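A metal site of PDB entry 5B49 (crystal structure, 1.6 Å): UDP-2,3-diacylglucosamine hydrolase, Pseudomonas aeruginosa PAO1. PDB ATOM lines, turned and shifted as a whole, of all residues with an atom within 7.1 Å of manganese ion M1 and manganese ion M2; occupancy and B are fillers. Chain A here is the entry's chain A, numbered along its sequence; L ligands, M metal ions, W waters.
An oxygen (O8) of the ligand sits at hydrogen-bond distance from a ring nitrogen (NE2) of His 195 (2.8 Å).
The guanidinium group of Arg 80 is in salt-bridge range of an oxygen (O1) of the ligand.
O1 of the ligand lies within hydrogen-bond range of ND2 of Asn 79 (2.6 Å).
Of the 20 residues printed, 4 come within 4 Å of manganese ion M1.
Along chain A the residues within 4 Å of manganese ion M1 span positions 8 to 197.
Of the 20 residues printed, 5 come within 4 Å of manganese ion M2.
The nearest printed residue that does not touch manganese ion M2 is Asp 116 (5.1 Å).
OD2 of Asp 8 lies within hydrogen-bond range of OG of Ser 7.
N of Gly 194 sits at hydrogen-bond distance from O of His 114, at 2.8 Å.
N of His 10 is in hydrogen-bond range of O of Phe 42 (3.3 Å).
N of His 195 sits at hydrogen-bond distance from OD2 of Asp 8, at 2.8 Å.
The side-chain carboxylate (OD1) of Asp 41 is in hydrogen-bond range of the backbone NH (N) of Arg 80 (2.9 Å).
A ring nitrogen (ND1) of His 114 sits at hydrogen-bond distance from the backbone carbonyl oxygen of Leu 39, 2.8 Å away.
O of Gly 40 sits at hydrogen-bond distance from N of Asp 8, 3.0 Å away.
The backbone carbonyl oxygen of Asp 41 is in hydrogen-bond range of the backbone NH of Leu 9, at 3.0 Å.
Manganese ion M2 is bound by OD1 of Asn 79.
Manganese ion M2 is bound by water W2.
Manganese ion M2 is bound by OD2 of Asp 41, at 2.2 Å.
Manganese ion M2 is bound by a ring nitrogen (NE2) of His 114 (2.2 Å).
ND1 of His 195 is bound to manganese ion M2.
Water W1 bridges O2 of the ligand (3.0 Å) and NH2 of Arg 80 (3.2 Å).
Water W2 lies within hydrogen-bond range of the backbone carbonyl oxygen (O) of His 195 and an oxygen (O2) of the ligand.
Manganese ion M1 is bound by OD1 of Asp 8.
Water W1 is bound to manganese ion M1 (2.2 Å).
A ring nitrogen (NE2) of His 10 is bound to manganese ion M1, 2.3 Å away.
Water W2 binds manganese ion M1, at 2.3 Å.
Manganese ion M1 is bound by NE2 of His 197 (2.3 Å).
The side-chain carboxylate (OD2) of Asp 41 is bound to manganese ion M1, 2.3 Å away.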
ATOM      1  N   SER A   7       6.468  10.787  24.753  1.00  0.00           N
ATOM      2  CA  SER A   7       6.666  12.202  25.068  1.00  0.00           C
ATOM      3  C   SER A   7       6.280  12.417  26.505  1.00  0.00           C
ATOM      4  O   SER A   7       5.659  11.576  27.150  1.00  0.00           O
ATOM      5  CB  SER A   7       5.859  13.142  24.165  1.00  0.00           C
ATOM      6  OG  SER A   7       4.481  13.019  24.373  1.00  0.00           O
ATOM      7  N   ASP A   8       6.596  13.615  27.013  1.00  0.00           N
ATOM      8  CA  ASP A   8       6.039  14.065  28.288  1.00  0.00           C
ATOM      9  C   ASP A   8       6.405  13.099  29.414  1.00  0.00           C
ATOM     10  O   ASP A   8       5.579  12.696  30.247  1.00  0.00           O
ATOM     11  CB  ASP A   8       4.526  14.298  28.174  1.00  0.00           C
ATOM     12  CG  ASP A   8       4.191  15.416  27.207  1.00  0.00           C
ATOM     13  OD1 ASP A   8       4.344  16.612  27.579  1.00  0.00           O
ATOM     14  OD2 ASP A   8       3.797  15.105  26.059  1.00  0.00           O
ATOM     15  N   LEU A   9       7.689  12.732  29.437  1.00  0.00           N
ATOM     16  CA  LEU A   9       8.225  11.956  30.541  1.00  0.00           C
ATOM     17  C   LEU A   9       8.629  12.857  31.711  1.00  0.00           C
ATOM     18  O   LEU A   9       8.514  12.439  32.859  1.00  0.00           O
ATOM     19  CB  LEU A   9       9.435  11.131  30.099  1.00  0.00           C
ATOM     20  CG  LEU A   9       9.145   9.932  29.199  1.00  0.00           C
ATOM     21  CD1 LEU A   9       8.925  10.356  27.756  1.00  0.00           C
ATOM     22  CD2 LEU A   9      10.295   8.947  29.269  1.00  0.00           C
ATOM     23  N   HIS A  10       9.114  14.079  31.411  1.00  0.00           N
ATOM     24  CA  HIS A  10       9.548  15.045  32.429  1.00  0.00           C
ATOM     25  C   HIS A  10      10.570  14.425  33.379  1.00  0.00           C
ATOM     26  O   HIS A  10      10.486  14.590  34.598  1.00  0.00           O
ATOM     27  CB  HIS A  10       8.346  15.594  33.208  1.00  0.00           C
ATOM     28  CG  HIS A  10       7.156  15.905  32.326  1.00  0.00           C
ATOM     29  ND1 HIS A  10       6.047  15.102  32.285  1.00  0.00           N
ATOM     30  CD2 HIS A  10       6.945  16.878  31.403  1.00  0.00           C
ATOM     31  CE1 HIS A  10       5.170  15.586  31.411  1.00  0.00           C
ATOM     32  NE2 HIS A  10       5.709  16.652  30.845  1.00  0.00           N
ATOM     33  N   LEU A  39       8.781  13.055  21.498  1.00  0.00           N
ATOM     34  CA  LEU A  39       8.170  14.291  20.998  1.00  0.00           C
ATOM     35  C   LEU A  39       8.030  15.342  22.087  1.00  0.00           C
ATOM     36  O   LEU A  39       6.941  15.911  22.308  1.00  0.00           O
ATOM     37  CB  LEU A  39       6.827  13.995  20.347  1.00  0.00           C
ATOM     38  CG  LEU A  39       6.872  12.974  19.203  1.00  0.00           C
ATOM     39  CD1 LEU A  39       5.485  12.898  18.543  1.00  0.00           C
ATOM     40  CD2 LEU A  39       7.952  13.289  18.171  1.00  0.00           C
ATOM     41  N   GLY A  40       9.123  15.669  22.750  1.00  0.00           N
ATOM     42  CA  GLY A  40       9.172  16.839  23.613  1.00  0.00           C
ATOM     43  C   GLY A  40       8.850  16.524  25.060  1.00  0.00           C
ATOM     44  O   GLY A  40       8.193  15.545  25.395  1.00  0.00           O
ATOM     45  N   ASP A  41       9.317  17.407  25.930  1.00  0.00           N
ATOM     46  CA  ASP A  41       9.130  17.299  27.387  1.00  0.00           C
ATOM     47  C   ASP A  41       9.724  15.978  27.873  1.00  0.00           C
ATOM     48  O   ASP A  41       9.138  15.261  28.708  1.00  0.00           O
ATOM     49  CB  ASP A  41       7.678  17.444  27.793  1.00  0.00           C
ATOM     50  CG  ASP A  41       7.168  18.890  27.724  1.00  0.00           C
ATOM     51  OD1 ASP A  41       7.915  19.784  27.263  1.00  0.00           O
ATOM     52  OD2 ASP A  41       6.000  19.072  28.098  1.00  0.00           O
ATOM     53  N   PHE A  42      10.874  15.638  27.294  1.00  0.00           N
ATOM     54  CA  PHE A  42      11.622  14.456  27.709  1.00  0.00           C
ATOM     55  C   PHE A  42      12.179  14.633  29.109  1.00  0.00           C
ATOM     56  O   PHE A  42      12.065  13.740  29.957  1.00  0.00           O
ATOM     57  CB  PHE A  42      12.721  14.195  26.682  1.00  0.00           C
ATOM     58  CG  PHE A  42      13.550  12.970  26.916  1.00  0.00           C
ATOM     59  CD1 PHE A  42      12.971  11.716  27.103  1.00  0.00           C
ATOM     60  CD2 PHE A  42      14.911  13.053  26.843  1.00  0.00           C
ATOM     61  CE1 PHE A  42      13.764  10.580  27.262  1.00  0.00           C
ATOM     62  CE2 PHE A  42      15.727  11.923  26.997  1.00  0.00           C
ATOM     63  CZ  PHE A  42      15.142  10.687  27.196  1.00  0.00           C
ATOM     64  N   GLY A  78      10.343  20.019  23.359  1.00  0.00           N
ATOM     65  CA  GLY A  78       9.077  20.410  23.952  1.00  0.00           C
ATOM     66  C   GLY A  78       9.197  21.742  24.644  1.00  0.00           C
ATOM     67  O   GLY A  78      10.229  22.406  24.541  1.00  0.00           O
ATOM     68  N   ASN A  79       8.197  22.157  25.385  1.00  0.00           N
ATOM     69  CA  ASN A  79       8.343  23.462  25.991  1.00  0.00           C
ATOM     70  C   ASN A  79       9.186  23.423  27.257  1.00  0.00           C
ATOM     71  O   ASN A  79       9.659  24.475  27.688  1.00  0.00           O
ATOM     72  CB  ASN A  79       6.981  24.064  26.253  1.00  0.00           C
ATOM     73  CG  ASN A  79       6.140  23.192  27.071  1.00  0.00           C
ATOM     74  OD1 ASN A  79       5.657  22.168  26.589  1.00  0.00           O
ATOM     75  ND2 ASN A  79       5.999  23.532  28.329  1.00  0.00           N
ATOM     76  N   ARG A  80       9.437  22.241  27.814  1.00  0.00           N
ATOM     77  CA  ARG A  80      10.366  22.119  28.933  1.00  0.00           C
ATOM     78  C   ARG A  80      11.809  22.101  28.483  1.00  0.00           C
ATOM     79  O   ARG A  80      12.697  22.495  29.256  1.00  0.00           O
ATOM     80  CB  ARG A  80      10.105  20.833  29.721  1.00  0.00           C
ATOM     81  CG  ARG A  80       8.775  20.779  30.376  1.00  0.00           C
ATOM     82  CD  ARG A  80       8.575  21.892  31.375  1.00  0.00           C
ATOM     83  NE  ARG A  80       7.312  21.677  32.068  1.00  0.00           N
ATOM     84  CZ  ARG A  80       7.117  20.812  33.050  1.00  0.00           C
ATOM     85  NH1 ARG A  80       8.115  20.058  33.531  1.00  0.00           N
ATOM     86  NH2 ARG A  80       5.901  20.668  33.565  1.00  0.00           N
ATOM     87  N   HIS A 114       5.451  18.754  19.227  1.00  0.00           N
ATOM     88  CA  HIS A 114       5.218  18.583  20.646  1.00  0.00           C
ATOM     89  C   HIS A 114       3.741  18.802  20.973  1.00  0.00           C
ATOM     90  O   HIS A 114       3.168  18.043  21.748  1.00  0.00           O
ATOM     91  CB  HIS A 114       6.103  19.499  21.482  1.00  0.00           C
ATOM     92  CG  HIS A 114       5.839  19.369  22.960  1.00  0.00           C
ATOM     93  ND1 HIS A 114       5.925  18.172  23.622  1.00  0.00           N
ATOM     94  CD2 HIS A 114       5.404  20.269  23.871  1.00  0.00           C
ATOM     95  CE1 HIS A 114       5.591  18.334  24.889  1.00  0.00           C
ATOM     96  NE2 HIS A 114       5.273  19.606  25.063  1.00  0.00           N
ATOM     97  N   GLY A 115       3.125  19.816  20.379  1.00  0.00           N
ATOM     98  CA  GLY A 115       1.705  20.056  20.561  1.00  0.00           C
ATOM     99  C   GLY A 115       1.384  21.419  21.134  1.00  0.00           C
ATOM    100  O   GLY A 115       0.258  21.912  20.929  1.00  0.00           O
ATOM    101  N   ASP A 116       2.330  22.046  21.825  1.00  0.00           N
ATOM    102  CA  ASP A 116       2.005  23.312  22.492  1.00  0.00           C
ATOM    103  C   ASP A 116       1.781  24.420  21.476  1.00  0.00           C
ATOM    104  O   ASP A 116       1.051  25.358  21.768  1.00  0.00           O
ATOM    105  CB  ASP A 116       3.105  23.704  23.468  1.00  0.00           C
ATOM    106  CG  ASP A 116       4.420  23.926  22.801  1.00  0.00           C
ATOM    107  OD1 ASP A 116       4.910  22.993  22.124  1.00  0.00           O
ATOM    108  OD2 ASP A 116       5.002  25.035  22.965  1.00  0.00           O
ATOM    109  N   TYR A 125       0.192  32.096  27.027  1.00  0.00           N
ATOM    110  CA  TYR A 125       1.248  31.154  26.675  1.00  0.00           C
ATOM    111  C   TYR A 125       1.781  31.436  25.279  1.00  0.00           C
ATOM    112  O   TYR A 125       2.997  31.372  25.050  1.00  0.00           O
ATOM    113  CB  TYR A 125       0.751  29.702  26.776  1.00  0.00           C
ATOM    114  CG  TYR A 125       1.865  28.809  26.270  1.00  0.00           C
ATOM    115  CD1 TYR A 125       3.077  28.798  26.925  1.00  0.00           C
ATOM    116  CD2 TYR A 125       1.735  28.096  25.082  1.00  0.00           C
ATOM    117  CE1 TYR A 125       4.145  28.078  26.450  1.00  0.00           C
ATOM    118  CE2 TYR A 125       2.814  27.349  24.595  1.00  0.00           C
ATOM    119  CZ  TYR A 125       4.014  27.358  25.290  1.00  0.00           C
ATOM    120  OH  TYR A 125       5.115  26.652  24.864  1.00  0.00           O
ATOM    121  N   GLY A 194       2.282  15.421  21.620  1.00  0.00           N
ATOM    122  CA  GLY A 194       2.078  15.258  23.042  1.00  0.00           C
ATOM    123  C   GLY A 194       1.570  16.541  23.655  1.00  0.00           C
ATOM    124  O   GLY A 194       0.552  17.099  23.207  1.00  0.00           O
ATOM    125  N   HIS A 195       2.270  17.020  24.694  1.00  0.00           N
ATOM    126  CA  HIS A 195       2.036  18.281  25.399  1.00  0.00           C
ATOM    127  C   HIS A 195       0.780  18.298  26.270  1.00  0.00           C
ATOM    128  O   HIS A 195       0.851  18.740  27.414  1.00  0.00           O
ATOM    129  CB  HIS A 195       1.972  19.500  24.467  1.00  0.00           C
ATOM    130  CG  HIS A 195       1.771  20.775  25.220  1.00  0.00           C
ATOM    131  ND1 HIS A 195       2.708  21.265  26.119  1.00  0.00           N
ATOM    132  CD2 HIS A 195       0.720  21.629  25.283  1.00  0.00           C
ATOM    133  CE1 HIS A 195       2.235  22.371  26.684  1.00  0.00           C
ATOM    134  NE2 HIS A 195       1.043  22.616  26.172  1.00  0.00           N
ATOM    135  N   THR A 196      -0.371  17.892  25.731  1.00  0.00           N
ATOM    136  CA  THR A 196      -1.632  18.112  26.445  1.00  0.00           C
ATOM    137  C   THR A 196      -1.913  17.088  27.533  1.00  0.00           C
ATOM    138  O   THR A 196      -2.835  17.301  28.317  1.00  0.00           O
ATOM    139  CB  THR A 196      -2.803  18.119  25.464  1.00  0.00           C
ATOM    140  OG1 THR A 196      -2.884  16.855  24.826  1.00  0.00           O
ATOM    141  CG2 THR A 196      -2.640  19.235  24.429  1.00  0.00           C
ATOM    142  N   HIS A 197      -1.145  15.994  27.585  1.00  0.00           N
ATOM    143  CA  HIS A 197      -1.256  14.986  28.639  1.00  0.00           C
ATOM    144  C   HIS A 197      -2.649  14.334  28.637  1.00  0.00           C
ATOM    145  O   HIS A 197      -3.164  13.927  29.670  1.00  0.00           O
ATOM    146  CB  HIS A 197      -0.973  15.557  30.025  1.00  0.00           C
ATOM    147  CG  HIS A 197       0.418  16.085  30.202  1.00  0.00           C
ATOM    148  ND1 HIS A 197       0.896  16.488  31.440  1.00  0.00           N
ATOM    149  CD2 HIS A 197       1.434  16.295  29.331  1.00  0.00           C
ATOM    150  CE1 HIS A 197       2.141  16.911  31.311  1.00  0.00           C
ATOM    151  NE2 HIS A 197       2.493  16.799  30.042  1.00  0.00           N
ATOM    152  N   ASP A 218       1.395  11.295  29.149  1.00  0.00           N
ATOM    153  CA  ASP A 218       2.475  11.705  30.034  1.00  0.00           C
ATOM    154  C   ASP A 218       2.716  10.617  31.069  1.00  0.00           C
ATOM    155  O   ASP A 218       1.843   9.785  31.336  1.00  0.00           O
ATOM    156  CB  ASP A 218       2.127  13.010  30.731  1.00  0.00           C
ATOM    157  CG  ASP A 218       1.024  12.832  31.751  1.00  0.00           C
ATOM    158  OD1 ASP A 218      -0.140  12.668  31.326  1.00  0.00           O
ATOM    159  OD2 ASP A 218       1.327  12.829  32.953  1.00  0.00           O
HETATM  160  O1  LIG L   1       5.334  23.203  30.776  1.00  0.00           O
HETATM  161  P1  LIG L   1       3.918  22.720  30.965  1.00  0.00           P
HETATM  162  O2  LIG L   1       3.488  21.797  29.869  1.00  0.00           O
HETATM  163  O3  LIG L   1       3.568  22.295  32.363  1.00  0.00           O
HETATM  164  O4  LIG L   1       3.011  24.091  30.841  1.00  0.00           O
HETATM  165  C1  LIG L   1       3.017  24.741  29.576  1.00  0.00           C
HETATM  166  C2  LIG L   1       3.164  26.250  29.736  1.00  0.00           C
HETATM  167  N1  LIG L   1       4.358  26.615  30.507  1.00  0.00           N
HETATM  168  C3  LIG L   1       5.563  26.707  29.965  1.00  0.00           C
HETATM  169  C4  LIG L   1       6.669  27.115  30.945  1.00  0.00           C
HETATM  170  C5  LIG L   1       7.584  25.918  31.226  1.00  0.00           C
HETATM  171  O5  LIG L   1       6.885  25.070  32.113  1.00  0.00           O
HETATM  172  C6  LIG L   1       8.904  26.358  31.888  1.00  0.00           C
HETATM  173  C7  LIG L   1      10.099  25.523  31.384  1.00  0.00           C
HETATM  174  C8  LIG L   1      11.473  26.092  31.723  1.00  0.00           C
HETATM  175  C9  LIG L   1      12.578  25.610  30.767  1.00  0.00           C
HETATM  176  C10 LIG L   1      13.304  26.721  30.022  1.00  0.00           C
HETATM  177  C11 LIG L   1      14.261  27.520  30.892  1.00  0.00           C
HETATM  178  C12 LIG L   1      14.606  28.836  30.187  1.00  0.00           C
HETATM  179  C13 LIG L   1      15.147  29.898  31.116  1.00  0.00           C
HETATM  180  C14 LIG L   1      16.326  29.419  31.929  1.00  0.00           C
HETATM  181  C15 LIG L   1      17.380  28.727  31.083  1.00  0.00           C
HETATM  182  C16 LIG L   1      17.891  29.587  29.959  1.00  0.00           C
HETATM  183  O6  LIG L   1       5.773  26.523  28.790  1.00  0.00           O
HETATM  184  C17 LIG L   1       1.950  26.852  30.396  1.00  0.00           C
HETATM  185  C18 LIG L   1       0.688  26.383  29.714  1.00  0.00           C
HETATM  186  C19 LIG L   1       0.654  24.878  29.625  1.00  0.00           C
HETATM  187  O7  LIG L   1       1.802  24.412  28.922  1.00  0.00           O
HETATM  188  C20 LIG L   1      -0.583  24.352  28.880  1.00  0.00           C
HETATM  189  O8  LIG L   1      -0.482  24.628  27.459  1.00  0.00           O
HETATM  190  O9  LIG L   1      -0.435  26.837  30.503  1.00  0.00           O
HETATM  191  O10 LIG L   1       2.092  28.227  30.161  1.00  0.00           O
HETATM  192  C21 LIG L   1       1.860  29.143  31.215  1.00  0.00           C
HETATM  193  O11 LIG L   1       1.299  28.779  32.242  1.00  0.00           O
HETATM  194  C22 LIG L   1       2.362  30.532  30.954  1.00  0.00           C
HETATM  195  C23 LIG L   1       1.615  31.597  31.732  1.00  0.00           C
HETATM  196  O12 LIG L   1       0.291  31.672  31.160  1.00  0.00           O
HETATM  197  C24 LIG L   1       2.325  32.954  31.625  1.00  0.00           C
HETATM  198  C25 LIG L   1       3.583  32.966  32.454  1.00  0.00           C
HETATM  199  C26 LIG L   1       4.436  34.239  32.347  1.00  0.00           C
HETATM  200  C27 LIG L   1       5.600  34.063  33.332  1.00  0.00           C
HETATM  201  C28 LIG L   1       6.604  35.194  33.351  1.00  0.00           C
HETATM  202  C29 LIG L   1       7.630  34.936  34.442  1.00  0.00           C
HETATM  203  C30 LIG L   1       8.763  35.955  34.541  1.00  0.00           C
HETATM  204  C31 LIG L   1       8.201  37.339  34.776  1.00  0.00           C
HETATM  205  C32 LIG L   1       9.243  38.231  35.423  1.00  0.00           C
HETATM  206  C33 LIG L   1       8.989  39.718  35.141  1.00  0.00           C
HETATM  207  C34 LIG L   1       9.540  40.562  36.252  1.00  0.00           C
HETATM  208 MN    MN M   1       4.475  17.826  29.370  1.00  0.00          MN
HETATM  209 MN    MN M   2       4.613  20.402  27.031  1.00  0.00          MN
HETATM  210  O   HOH W   1       4.470  19.241  31.108  1.00  0.00           O
HETATM  211  O   HOH W   2       3.218  19.461  28.436  1.00  0.00           O
